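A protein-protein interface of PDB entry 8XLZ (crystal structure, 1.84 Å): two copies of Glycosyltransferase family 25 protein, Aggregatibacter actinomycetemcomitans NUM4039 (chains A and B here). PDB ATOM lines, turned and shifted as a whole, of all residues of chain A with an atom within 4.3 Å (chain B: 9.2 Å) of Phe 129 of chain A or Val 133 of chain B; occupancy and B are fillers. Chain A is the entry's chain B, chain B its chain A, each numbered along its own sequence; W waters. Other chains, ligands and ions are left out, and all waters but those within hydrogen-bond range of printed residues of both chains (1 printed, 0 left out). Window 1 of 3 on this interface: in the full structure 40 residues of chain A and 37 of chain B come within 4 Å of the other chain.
Met 131 of chain A touches Leu 130 of chain B, but with the chains exchanged Leu 130 of chain A does not touch Met 131 of chain B (6.0 Å). Met 131 of chain A touches its own counterpart, Met 131 of chain B. Trp 157 of chain A touches Met 131 of chain B, but with the chains exchanged Met 131 of chain A does not touch Trp 157 of chain B (7.1 Å). Positions printed for both chains: 129, 130, 131 and 157. Of the 20 pairs that touch across the chains among the printed residues, 1 has its exchanged pair printed and touching as well.
Among the printed residues, pairs that only touch across the chains: Phe 192 of chain A with Pro 132 of chain B (3.2 Å), Phe 129 of chain A with Leu 135 of chain B (3.3 Å), Arg 125 of chain A with Leu 152 of chain B (3.3 Å), Met 131 of chain A with Leu 130 of chain B (3.5 Å), Asn 207 of chain A with Leu 135 of chain B (3.5 Å), Asn 207 of chain A with Arg 147 of chain B (3.6 Å), Trp 157 of chain A with Val 133 of chain B (3.7 Å), Asn 207 of chain A with Lys 137 of chain B (3.7 Å), Trp 157 of chain A with Leu 152 of chain B (3.8 Å), Gln 205 of chain A with Leu 152 of chain B (3.8 Å), Phe 129 of chain A with Val 133 of chain B (3.8 Å), Phe 192 of chain A with Val 133 of chain B (3.8 Å), Trp 157 of chain A with Met 131 of chain B (3.97 Å) and Phe 192 of chain A with Met 131 of chain B (3.98 Å).
Printed residues of chain B that touch a printed residue of chain A: Leu 130, Met 131, Pro 132, Val 133, Leu 135, Lys 137, Arg 147, Asp 148, Asp 150, Leu 152 and Ser 154. Hydrophobic or aromatic side chains of chain B within 4 Å of the printed part of chain A: Leu 130, Met 131, Pro 132, Val 133, Leu 135 and Leu 152. Among the printed residues, no Asp or Glu carboxylate lies within 4 Å of a Lys or Arg side-chain nitrogen of the other chain.
The backbone NH (N) of Met 131 of chain B is in hydrogen-bond range of the backbone carbonyl oxygen (O) of Met 131 of chain A. The backbone NH of Asp 148 of chain B is in hydrogen-bond range of the backbone carbonyl oxygen of Asn 207 of chain A, 2.9 Å away. O of Asp 150 of chain B lies within hydrogen-bond range of N of Gln 205 of chain A (2.8 Å). The side-chain carboxylate of Asp 150 of chain B lies within hydrogen-bond range of the side-chain amide nitrogen of Asn 207 of chain A. The side-chain hydroxyl (OG) of Ser 154 of chain B is in hydrogen-bond range of the backbone carbonyl oxygen (O) of Phe 192 of chain A, at 2.6 Å. O of Gln 205 of chain A lies close to O of Asp 148 of chain B (3.5 Å).
Phe 129 of chain A touches just these residues of chain B: Val 133 and Leu 135. Val 133 of chain B touches just these residues of chain A: Phe 129, Trp 157 and Phe 192. No residue of chain B comes within 4 Å of Thr 128 of chain A. No residue of chain B comes within 4 Å of Leu 130 of chain A. Of the printed residues of chain A, Leu 135 of chain B touches Phe 129 (3.3 Å) and Asn 207 (3.5 Å). Of the printed residues of chain B, Asn 207 of chain A touches Leu 135 (3.5 Å), Lys 137 (3.7 Å), Arg 147 (3.6 Å), Asp 148 (2.9 Å) and Asp 150 (2.8 Å). Val 216 of chain B touches none of the printed residues of chain A. Phe 129 of chain B touches none of the printed residues of chain A. The nearest residue of chain B that does not touch Phe 129 of chain A is Leu 152 of chain B (4.7 Å). The nearest printed residue of chain A that does not touch Ser 154 of chain B is Trp 157 of chain A (6.1 Å).
Water W1 lies within hydrogen-bond range of the backbone carbonyl oxygen (O) of Phe 129 of chain A (2.7 Å), the backbone carbonyl oxygen (O) of Met 131 of chain B (2.8 Å) and the backbone NH (N) of Met 131 of chain A (3.1 Å).
The side-chain carboxylate (OD2) of Asp 150 of chain B is in salt-bridge range of the side-chain amino group (NZ) of Lys 137 of chain B. NH1 of Arg 125 of chain A lies within hydrogen-bond range of O of Thr 128 of chain A, at 3.0 Å. The backbone carbonyl oxygen (O) of Glu 127 of chain A lies within hydrogen-bond range of the side-chain amide nitrogen (NE2) of Gln 205 of chain A, at 2.8 Å.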
ATOM      1  N   ARG A 125     -14.285  19.108   9.629  1.00  0.00           N
ATOM      2  CA  ARG A 125     -15.083  18.710   8.477  1.00  0.00           C
ATOM      3  C   ARG A 125     -16.114  19.787   8.215  1.00  0.00           C
ATOM      4  O   ARG A 125     -16.787  20.249   9.128  1.00  0.00           O
ATOM      5  CB  ARG A 125     -15.808  17.415   8.738  1.00  0.00           C
ATOM      6  CG  ARG A 125     -14.933  16.219   9.121  1.00  0.00           C
ATOM      7  CD  ARG A 125     -15.732  14.908   9.053  1.00  0.00           C
ATOM      8  NE  ARG A 125     -16.019  14.447   7.688  1.00  0.00           N
ATOM      9  CZ  ARG A 125     -17.199  14.502   7.070  1.00  0.00           C
ATOM     10  NH1 ARG A 125     -18.260  14.993   7.687  1.00  0.00           N
ATOM     11  NH2 ARG A 125     -17.315  14.044   5.827  1.00  0.00           N
ATOM     12  N   GLU A 127     -18.336  19.381   5.380  1.00  0.00           N
ATOM     13  CA  GLU A 127     -19.443  18.738   4.694  1.00  0.00           C
ATOM     14  C   GLU A 127     -20.339  17.953   5.659  1.00  0.00           C
ATOM     15  O   GLU A 127     -20.003  17.755   6.837  1.00  0.00           O
ATOM     16  CB  GLU A 127     -18.934  17.853   3.563  1.00  0.00           C
ATOM     17  CG  GLU A 127     -18.483  16.456   3.942  1.00  0.00           C
ATOM     18  CD  GLU A 127     -18.037  15.622   2.738  1.00  0.00           C
ATOM     19  OE1 GLU A 127     -18.828  15.209   1.858  1.00  0.00           O
ATOM     20  OE2 GLU A 127     -16.848  15.321   2.679  1.00  0.00           O
ATOM     21  N   THR A 128     -21.462  17.499   5.137  1.00  0.00           N
ATOM     22  CA  THR A 128     -22.452  16.773   5.918  1.00  0.00           C
ATOM     23  C   THR A 128     -21.845  15.547   6.576  1.00  0.00           C
ATOM     24  O   THR A 128     -20.862  15.000   6.100  1.00  0.00           O
ATOM     25  CB  THR A 128     -23.637  16.319   5.032  1.00  0.00           C
ATOM     26  OG1 THR A 128     -23.149  15.575   3.905  1.00  0.00           O
ATOM     27  CG2 THR A 128     -24.394  17.536   4.498  1.00  0.00           C
ATOM     28  N   PHE A 129     -22.438  15.137   7.684  1.00  0.00           N
ATOM     29  CA  PHE A 129     -21.964  13.994   8.450  1.00  0.00           C
ATOM     30  C   PHE A 129     -22.978  12.842   8.464  1.00  0.00           C
ATOM     31  O   PHE A 129     -22.660  11.774   8.956  1.00  0.00           O
ATOM     32  CB  PHE A 129     -21.586  14.434   9.869  1.00  0.00           C
ATOM     33  CG  PHE A 129     -22.683  15.161  10.593  1.00  0.00           C
ATOM     34  CD1 PHE A 129     -23.631  14.454  11.334  1.00  0.00           C
ATOM     35  CD2 PHE A 129     -22.802  16.545  10.515  1.00  0.00           C
ATOM     36  CE1 PHE A 129     -24.670  15.114  11.977  1.00  0.00           C
ATOM     37  CE2 PHE A 129     -23.830  17.215  11.160  1.00  0.00           C
ATOM     38  CZ  PHE A 129     -24.767  16.502  11.895  1.00  0.00           C
ATOM     39  N   LEU A 130     -24.185  13.084   7.936  1.00  0.00           N
ATOM     40  CA  LEU A 130     -25.166  12.045   7.727  1.00  0.00           C
ATOM     41  C   LEU A 130     -25.028  11.562   6.314  1.00  0.00           C
ATOM     42  O   LEU A 130     -25.581  12.173   5.412  1.00  0.00           O
ATOM     43  CB  LEU A 130     -26.580  12.597   7.920  1.00  0.00           C
ATOM     44  CG  LEU A 130     -26.916  13.098   9.336  1.00  0.00           C
ATOM     45  CD1 LEU A 130     -28.350  13.615   9.317  1.00  0.00           C
ATOM     46  CD2 LEU A 130     -26.714  12.017  10.393  1.00  0.00           C
ATOM     47  N   MET A 131     -24.298  10.465   6.133  1.00  0.00           N
ATOM     48  CA  MET A 131     -23.961   9.933   4.807  1.00  0.00           C
ATOM     49  C   MET A 131     -24.340   8.458   4.741  1.00  0.00           C
ATOM     50  O   MET A 131     -23.896   7.667   5.586  1.00  0.00           O
ATOM     51  CB  MET A 131     -22.452  10.029   4.529  1.00  0.00           C
ATOM     52  CG  MET A 131     -21.856  11.401   4.834  1.00  0.00           C
ATOM     53  SD  MET A 131     -20.209  11.691   4.156  1.00  0.00           S
ATOM     54  CE  MET A 131     -20.457  13.343   3.548  1.00  0.00           C
ATOM     55  N   TRP A 157     -17.394   7.362   2.958  1.00  0.00           N
ATOM     56  CA  TRP A 157     -17.316   8.535   3.817  1.00  0.00           C
ATOM     57  C   TRP A 157     -16.843   9.733   2.992  1.00  0.00           C
ATOM     58  O   TRP A 157     -16.142   9.564   2.005  1.00  0.00           O
ATOM     59  CB  TRP A 157     -16.381   8.260   4.998  1.00  0.00           C
ATOM     60  CG  TRP A 157     -16.331   9.349   6.051  1.00  0.00           C
ATOM     61  CD1 TRP A 157     -15.227   9.995   6.473  1.00  0.00           C
ATOM     62  CD2 TRP A 157     -17.434   9.901   6.792  1.00  0.00           C
ATOM     63  NE1 TRP A 157     -15.545  10.891   7.455  1.00  0.00           N
ATOM     64  CE2 TRP A 157     -16.897  10.864   7.664  1.00  0.00           C
ATOM     65  CE3 TRP A 157     -18.802   9.647   6.825  1.00  0.00           C
ATOM     66  CZ2 TRP A 157     -17.688  11.607   8.553  1.00  0.00           C
ATOM     67  CZ3 TRP A 157     -19.595  10.380   7.693  1.00  0.00           C
ATOM     68  CH2 TRP A 157     -19.030  11.373   8.539  1.00  0.00           C
ATOM     69  N   PHE A 192     -12.007   7.852   7.929  1.00  0.00           N
ATOM     70  CA  PHE A 192     -13.129   7.442   8.802  1.00  0.00           C
ATOM     71  C   PHE A 192     -12.689   6.616  10.015  1.00  0.00           C
ATOM     72  O   PHE A 192     -13.131   6.869  11.133  1.00  0.00           O
ATOM     73  CB  PHE A 192     -14.166   6.603   8.048  1.00  0.00           C
ATOM     74  CG  PHE A 192     -15.418   6.387   8.824  1.00  0.00           C
ATOM     75  CD1 PHE A 192     -16.330   7.416   8.945  1.00  0.00           C
ATOM     76  CD2 PHE A 192     -15.687   5.160   9.445  1.00  0.00           C
ATOM     77  CE1 PHE A 192     -17.498   7.248   9.661  1.00  0.00           C
ATOM     78  CE2 PHE A 192     -16.842   4.987  10.191  1.00  0.00           C
ATOM     79  CZ  PHE A 192     -17.753   6.037  10.293  1.00  0.00           C
ATOM     80  N   GLN A 205     -16.475  18.634  13.591  1.00  0.00           N
ATOM     81  CA  GLN A 205     -17.519  18.700  12.597  1.00  0.00           C
ATOM     82  C   GLN A 205     -18.285  20.011  12.743  1.00  0.00           C
ATOM     83  O   GLN A 205     -18.800  20.307  13.828  1.00  0.00           O
ATOM     84  CB  GLN A 205     -18.500  17.554  12.812  1.00  0.00           C
ATOM     85  CG  GLN A 205     -19.709  17.546  11.878  1.00  0.00           C
ATOM     86  CD  GLN A 205     -19.306  17.354  10.422  1.00  0.00           C
ATOM     87  OE1 GLN A 205     -18.624  16.382  10.071  1.00  0.00           O
ATOM     88  NE2 GLN A 205     -19.691  18.295   9.576  1.00  0.00           N
ATOM     89  N   ASN A 207     -21.496  22.006  12.472  1.00  0.00           N
ATOM     90  CA  ASN A 207     -22.860  21.508  12.629  1.00  0.00           C
ATOM     91  C   ASN A 207     -23.869  22.646  12.844  1.00  0.00           C
ATOM     92  O   ASN A 207     -23.892  23.234  13.917  1.00  0.00           O
ATOM     93  CB  ASN A 207     -22.912  20.522  13.797  1.00  0.00           C
ATOM     94  CG  ASN A 207     -24.243  19.839  13.925  1.00  0.00           C
ATOM     95  OD1 ASN A 207     -25.131  20.042  13.107  1.00  0.00           O
ATOM     96  ND2 ASN A 207     -24.391  19.027  14.958  1.00  0.00           N
ATOM     97  N   PHE B 129     -28.936   2.710   7.455  1.00  0.00           N
ATOM     98  CA  PHE B 129     -27.669   2.409   6.789  1.00  0.00           C
ATOM     99  C   PHE B 129     -26.789   3.663   6.629  1.00  0.00           C
ATOM    100  O   PHE B 129     -26.008   3.785   5.679  1.00  0.00           O
ATOM    101  CB  PHE B 129     -27.900   1.711   5.433  1.00  0.00           C
ATOM    102  CG  PHE B 129     -28.871   2.407   4.534  1.00  0.00           C
ATOM    103  CD1 PHE B 129     -30.225   2.104   4.597  1.00  0.00           C
ATOM    104  CD2 PHE B 129     -28.434   3.335   3.593  1.00  0.00           C
ATOM    105  CE1 PHE B 129     -31.141   2.745   3.748  1.00  0.00           C
ATOM    106  CE2 PHE B 129     -29.343   3.965   2.741  1.00  0.00           C
ATOM    107  CZ  PHE B 129     -30.694   3.688   2.838  1.00  0.00           C
ATOM    108  N   LEU B 130     -26.858   4.575   7.587  1.00  0.00           N
ATOM    109  CA  LEU B 130     -25.944   5.724   7.599  1.00  0.00           C
ATOM    110  C   LEU B 130     -24.584   5.296   8.150  1.00  0.00           C
ATOM    111  O   LEU B 130     -24.509   4.402   8.974  1.00  0.00           O
ATOM    112  CB  LEU B 130     -26.505   6.860   8.411  1.00  0.00           C
ATOM    113  CG  LEU B 130     -27.854   7.407   7.930  1.00  0.00           C
ATOM    114  CD1 LEU B 130     -28.393   8.430   8.928  1.00  0.00           C
ATOM    115  CD2 LEU B 130     -27.754   7.998   6.540  1.00  0.00           C
ATOM    116  N   MET B 131     -23.517   5.901   7.650  1.00  0.00           N
ATOM    117  CA  MET B 131     -22.201   5.693   8.243  1.00  0.00           C
ATOM    118  C   MET B 131     -22.247   5.938   9.757  1.00  0.00           C
ATOM    119  O   MET B 131     -22.883   6.889  10.222  1.00  0.00           O
ATOM    120  CB  MET B 131     -21.171   6.549   7.555  1.00  0.00           C
ATOM    121  CG  MET B 131     -20.909   6.056   6.143  1.00  0.00           C
ATOM    122  SD  MET B 131     -20.056   4.471   6.068  1.00  0.00           S
ATOM    123  CE  MET B 131     -18.390   4.935   6.517  1.00  0.00           C
ATOM    124  N   PRO B 132     -21.607   5.042  10.541  1.00  0.00           N
ATOM    125  CA  PRO B 132     -21.772   5.088  11.979  1.00  0.00           C
ATOM    126  C   PRO B 132     -20.906   6.162  12.625  1.00  0.00           C
ATOM    127  O   PRO B 132     -19.697   6.011  12.832  1.00  0.00           O
ATOM    128  CB  PRO B 132     -21.376   3.687  12.424  1.00  0.00           C
ATOM    129  CG  PRO B 132     -20.375   3.274  11.409  1.00  0.00           C
ATOM    130  CD  PRO B 132     -20.840   3.858  10.119  1.00  0.00           C
ATOM    131  N   VAL B 133     -21.566   7.211  13.047  1.00  0.00           N
ATOM    132  CA  VAL B 133     -20.895   8.398  13.493  1.00  0.00           C
ATOM    133  C   VAL B 133     -21.530   8.891  14.782  1.00  0.00           C
ATOM    134  O   VAL B 133     -22.713   8.676  14.996  1.00  0.00           O
ATOM    135  CB  VAL B 133     -20.943   9.357  12.274  1.00  0.00           C
ATOM    136  CG1 VAL B 133     -21.865  10.538  12.468  1.00  0.00           C
ATOM    137  CG2 VAL B 133     -19.545   9.652  11.824  1.00  0.00           C
ATOM    138  N   GLN B 134     -20.749   9.499  15.665  1.00  0.00           N
ATOM    139  CA  GLN B 134     -21.341  10.255  16.788  1.00  0.00           C
ATOM    140  C   GLN B 134     -20.680  11.618  17.071  1.00  0.00           C
ATOM    141  O   GLN B 134     -19.448  11.794  16.953  1.00  0.00           O
ATOM    142  CB  GLN B 134     -21.414   9.421  18.063  1.00  0.00           C
ATOM    143  CG  GLN B 134     -20.122   8.742  18.452  1.00  0.00           C
ATOM    144  CD  GLN B 134     -20.355   7.619  19.441  1.00  0.00           C
ATOM    145  OE1 GLN B 134     -21.362   7.626  20.164  1.00  0.00           O
ATOM    146  NE2 GLN B 134     -19.444   6.637  19.470  1.00  0.00           N
ATOM    147  N   LEU B 135     -21.543  12.560  17.438  1.00  0.00           N
ATOM    148  CA  LEU B 135     -21.179  13.943  17.690  1.00  0.00           C
ATOM    149  C   LEU B 135     -21.231  14.198  19.190  1.00  0.00           C
ATOM    150  O   LEU B 135     -22.235  13.904  19.806  1.00  0.00           O
ATOM    151  CB  LEU B 135     -22.153  14.873  16.967  1.00  0.00           C
ATOM    152  CG  LEU B 135     -22.175  14.760  15.439  1.00  0.00           C
ATOM    153  CD1 LEU B 135     -23.118  15.773  14.793  1.00  0.00           C
ATOM    154  CD2 LEU B 135     -20.787  14.945  14.876  1.00  0.00           C
ATOM    155  N   GLU B 136     -20.105  14.652  19.757  1.00  0.00           N
ATOM    156  CA  GLU B 136     -20.025  15.162  21.136  1.00  0.00           C
ATOM    157  C   GLU B 136     -20.016  16.683  21.072  1.00  0.00           C
ATOM    158  O   GLU B 136     -19.207  17.286  20.361  1.00  0.00           O
ATOM    159  CB  GLU B 136     -18.744  14.664  21.819  1.00  0.00           C
ATOM    160  CG  GLU B 136     -18.656  14.936  23.312  1.00  0.00           C
ATOM    161  CD  GLU B 136     -17.362  14.407  23.925  1.00  0.00           C
ATOM    162  OE1 GLU B 136     -16.827  13.390  23.450  1.00  0.00           O
ATOM    163  OE2 GLU B 136     -16.870  15.006  24.891  1.00  0.00           O
ATOM    164  N   LYS B 137     -20.935  17.301  21.804  1.00  0.00           N
ATOM    165  CA  LYS B 137     -20.950  18.747  21.942  1.00  0.00           C
ATOM    166  C   LYS B 137     -19.760  19.184  22.801  1.00  0.00           C
ATOM    167  O   LYS B 137     -19.261  18.424  23.617  1.00  0.00           O
ATOM    168  CB  LYS B 137     -22.251  19.191  22.609  1.00  0.00           C
ATOM    169  CG  LYS B 137     -23.496  18.890  21.799  1.00  0.00           C
ATOM    170  CD  LYS B 137     -23.495  19.720  20.536  1.00  0.00           C
ATOM    171  CE  LYS B 137     -24.857  19.792  19.871  1.00  0.00           C
ATOM    172  NZ  LYS B 137     -24.644  20.283  18.479  1.00  0.00           N
ATOM    173  N   ARG B 147     -23.147  28.071  13.861  1.00  0.00           N
ATOM    174  CA  ARG B 147     -22.790  26.671  13.646  1.00  0.00           C
ATOM    175  C   ARG B 147     -21.878  26.206  14.763  1.00  0.00           C
ATOM    176  O   ARG B 147     -20.896  26.862  15.096  1.00  0.00           O
ATOM    177  CB  ARG B 147     -22.158  26.487  12.273  1.00  0.00           C
ATOM    178  CG  ARG B 147     -23.065  27.078  11.228  1.00  0.00           C
ATOM    179  CD  ARG B 147     -22.662  26.753   9.829  1.00  0.00           C
ATOM    180  NE  ARG B 147     -23.478  27.517   8.893  1.00  0.00           N
ATOM    181  CZ  ARG B 147     -24.326  26.995   8.016  1.00  0.00           C
ATOM    182  NH1 ARG B 147     -24.494  25.682   7.921  1.00  0.00           N
ATOM    183  NH2 ARG B 147     -24.998  27.801   7.212  1.00  0.00           N
ATOM    184  N   ASP B 148     -22.227  25.072  15.343  1.00  0.00           N
ATOM    185  CA  ASP B 148     -21.450  24.468  16.399  1.00  0.00           C
ATOM    186  C   ASP B 148     -20.238  23.781  15.819  1.00  0.00           C
ATOM    187  O   ASP B 148     -20.210  23.392  14.649  1.00  0.00           O
ATOM    188  CB  ASP B 148     -22.289  23.439  17.156  1.00  0.00           C
ATOM    189  CG  ASP B 148     -23.240  24.080  18.156  1.00  0.00           C
ATOM    190  OD1 ASP B 148     -23.146  25.313  18.410  1.00  0.00           O
ATOM    191  OD2 ASP B 148     -24.061  23.330  18.710  1.00  0.00           O
ATOM    192  N   ASP B 150     -18.594  20.536  16.740  1.00  0.00           N
ATOM    193  CA  ASP B 150     -18.756  19.301  17.519  1.00  0.00           C
ATOM    194  C   ASP B 150     -17.566  18.429  17.319  1.00  0.00           C
ATOM    195  O   ASP B 150     -16.831  18.601  16.351  1.00  0.00           O
ATOM    196  CB  ASP B 150     -19.987  18.527  17.076  1.00  0.00           C
ATOM    197  CG  ASP B 150     -21.293  19.256  17.394  1.00  0.00           C
ATOM    198  OD1 ASP B 150     -21.290  20.238  18.184  1.00  0.00           O
ATOM    199  OD2 ASP B 150     -22.316  18.819  16.833  1.00  0.00           O
ATOM    200  N   ILE B 151     -17.387  17.480  18.216  1.00  0.00           N
ATOM    201  CA  ILE B 151     -16.311  16.498  18.122  1.00  0.00           C
ATOM    202  C   ILE B 151     -16.905  15.208  17.525  1.00  0.00           C
ATOM    203  O   ILE B 151     -17.897  14.642  18.036  1.00  0.00           O
ATOM    204  CB  ILE B 151     -15.699  16.216  19.483  1.00  0.00           C
ATOM    205  CG1 ILE B 151     -15.131  17.494  20.086  1.00  0.00           C
ATOM    206  CG2 ILE B 151     -14.601  15.160  19.397  1.00  0.00           C
ATOM    207  CD1 ILE B 151     -14.921  17.392  21.582  1.00  0.00           C
ATOM    208  N   LEU B 152     -16.317  14.790  16.412  1.00  0.00           N
ATOM    209  CA  LEU B 152     -16.828  13.696  15.619  1.00  0.00           C
ATOM    210  C   LEU B 152     -15.977  12.439  15.813  1.00  0.00           C
ATOM    211  O   LEU B 152     -14.767  12.427  15.587  1.00  0.00           O
ATOM    212  CB  LEU B 152     -16.802  14.070  14.146  1.00  0.00           C
ATOM    213  CG  LEU B 152     -17.294  13.012  13.170  1.00  0.00           C
ATOM    214  CD1 LEU B 152     -18.781  12.867  13.311  1.00  0.00           C
ATOM    215  CD2 LEU B 152     -16.982  13.438  11.752  1.00  0.00           C
ATOM    216  N   THR B 153     -16.630  11.361  16.203  1.00  0.00           N
ATOM    217  CA  THR B 153     -15.984  10.059  16.239  1.00  0.00           C
ATOM    218  C   THR B 153     -16.765   9.054  15.413  1.00  0.00           C
ATOM    219  O   THR B 153     -17.957   9.203  15.165  1.00  0.00           O
ATOM    220  CB  THR B 153     -15.862   9.500  17.649  1.00  0.00           C
ATOM    221  OG1 THR B 153     -17.124   9.655  18.303  1.00  0.00           O
ATOM    222  CG2 THR B 153     -14.760  10.239  18.414  1.00  0.00           C
ATOM    223  N   SER B 154     -16.054   8.018  14.990  1.00  0.00           N
ATOM    224  CA  SER B 154     -16.682   6.877  14.345  1.00  0.00           C
ATOM    225  C   SER B 154     -17.034   5.820  15.415  1.00  0.00           C
ATOM    226  O   SER B 154     -16.344   5.677  16.396  1.00  0.00           O
ATOM    227  CB  SER B 154     -15.732   6.290  13.315  1.00  0.00           C
ATOM    228  OG  SER B 154     -15.480   7.238  12.296  1.00  0.00           O
ATOM    229  N   MET B 155     -18.115   5.098  15.204  1.00  0.00           N
ATOM    230  CA  MET B 155     -18.443   3.929  16.008  1.00  0.00           C
ATOM    231  C   MET B 155     -18.703   2.714  15.102  1.00  0.00           C
ATOM    232  O   MET B 155     -18.655   2.804  13.875  1.00  0.00           O
ATOM    233  CB  MET B 155     -19.649   4.223  16.890  1.00  0.00           C
ATOM    234  CG  MET B 155     -20.832   4.808  16.154  1.00  0.00           C
ATOM    235  SD  MET B 155     -22.173   5.141  17.304  1.00  0.00           S
ATOM    236  CE  MET B 155     -23.559   5.246  16.156  1.00  0.00           C
ATOM    237  N   ASP B 156     -18.957   1.569  15.714  1.00  0.00           N
ATOM    238  CA  ASP B 156     -19.229   0.366  14.966  1.00  0.00           C
ATOM    239  C   ASP B 156     -20.553   0.548  14.221  1.00  0.00           C
ATOM    240  O   ASP B 156     -21.484   1.172  14.716  1.00  0.00           O
ATOM    241  CB  ASP B 156     -19.345  -0.830  15.902  1.00  0.00           C
ATOM    242  CG  ASP B 156     -18.019  -1.201  16.567  1.00  0.00           C
ATOM    243  OD1 ASP B 156     -16.939  -1.167  15.914  1.00  0.00           O
ATOM    244  OD2 ASP B 156     -18.095  -1.554  17.767  1.00  0.00           O
ATOM    245  N   TRP B 157     -20.640  -0.007  13.039  1.00  0.00           N
ATOM    246  CA  TRP B 157     -21.919  -0.005  12.335  1.00  0.00           C
ATOM    247  C   TRP B 157     -22.875  -0.990  13.010  1.00  0.00           C
ATOM    248  O   TRP B 157     -22.440  -1.922  13.700  1.00  0.00           O
ATOM    249  CB  TRP B 157     -21.720  -0.382  10.887  1.00  0.00           C
ATOM    250  CG  TRP B 157     -22.780   0.090   9.932  1.00  0.00           C
ATOM    251  CD1 TRP B 157     -23.498   1.260   9.977  1.00  0.00           C
ATOM    252  CD2 TRP B 157     -23.173  -0.565   8.727  1.00  0.00           C
ATOM    253  NE1 TRP B 157     -24.329   1.354   8.887  1.00  0.00           N
ATOM    254  CE2 TRP B 157     -24.137   0.256   8.092  1.00  0.00           C
ATOM    255  CE3 TRP B 157     -22.801  -1.767   8.114  1.00  0.00           C
ATOM    256  CZ2 TRP B 157     -24.741  -0.099   6.889  1.00  0.00           C
ATOM    257  CZ3 TRP B 157     -23.402  -2.118   6.920  1.00  0.00           C
ATOM    258  CH2 TRP B 157     -24.350  -1.279   6.310  1.00  0.00           C
ATOM    259  N   GLY B 158     -24.169  -0.784  12.781  1.00  0.00           N
ATOM    260  CA  GLY B 158     -25.208  -1.523  13.468  1.00  0.00           C
ATOM    261  C   GLY B 158     -25.307  -3.000  13.112  1.00  0.00           C
ATOM    262  O   GLY B 158     -25.111  -3.374  11.958  1.00  0.00           O
ATOM    263  N   LEU B 215     -29.941   5.226  19.815  1.00  0.00           N
ATOM    264  CA  LEU B 215     -28.819   6.181  19.745  1.00  0.00           C
ATOM    265  C   LEU B 215     -28.599   6.814  18.359  1.00  0.00           C
ATOM    266  O   LEU B 215     -28.177   7.971  18.281  1.00  0.00           O
ATOM    267  CB  LEU B 215     -27.516   5.509  20.215  1.00  0.00           C
ATOM    268  CG  LEU B 215     -26.302   6.422  20.489  1.00  0.00           C
ATOM    269  CD1 LEU B 215     -25.581   6.032  21.779  1.00  0.00           C
ATOM    270  CD2 LEU B 215     -25.331   6.459  19.311  1.00  0.00           C
ATOM    271  N   VAL B 216     -28.866   6.068  17.281  1.00  0.00           N
ATOM    272  CA  VAL B 216     -28.663   6.566  15.901  1.00  0.00           C
ATOM    273  C   VAL B 216     -29.712   7.615  15.485  1.00  0.00           C
ATOM    274  O   VAL B 216     -29.378   8.558  14.765  1.00  0.00           O
ATOM    275  CB  VAL B 216     -28.624   5.415  14.852  1.00  0.00           C
ATOM    276  CG1 VAL B 216     -28.502   5.963  13.429  1.00  0.00           C
ATOM    277  CG2 VAL B 216     -27.468   4.459  15.135  1.00  0.00           C
ATOM    278  N   LEU B 217     -30.961   7.448  15.932  1.00  0.00           N
ATOM    279  CA  LEU B 217     -32.028   8.458  15.722  1.00  0.00           C
ATOM    280  C   LEU B 217     -31.657   9.877  16.218  1.00  0.00           C
ATOM    281  O   LEU B 217     -32.189  10.871  15.712  1.00  0.00           O
ATOM    282  CB  LEU B 217     -33.353   8.036  16.413  1.00  0.00           C
ATOM    283  CG  LEU B 217     -34.608   7.629  15.613  1.00  0.00           C
ATOM    284  CD1 LEU B 217     -35.860   7.755  16.485  1.00  0.00           C
ATOM    285  CD2 LEU B 217     -34.804   8.421  14.320  1.00  0.00           C
ATOM    286  N   ASN B 218     -30.745   9.955  17.194  1.00  0.00           N
ATOM    287  CA  ASN B 218     -30.518  11.165  17.995  1.00  0.00           C
ATOM    288  C   ASN B 218     -29.452  12.106  17.412  1.00  0.00           C
ATOM    289  O   ASN B 218     -28.702  11.743  16.502  1.00  0.00           O
ATOM    290  CB  ASN B 218     -30.121  10.771  19.431  1.00  0.00           C
ATOM    291  CG  ASN B 218     -31.233  10.050  20.200  1.00  0.00           C
ATOM    292  OD1 ASN B 218     -31.277  10.135  21.421  1.00  0.00           O
ATOM    293  ND2 ASN B 218     -32.115   9.335  19.510  1.00  0.00           N
HETATM  294  O   HOH W   1     -23.562   9.244   8.846  1.00  0.00           O
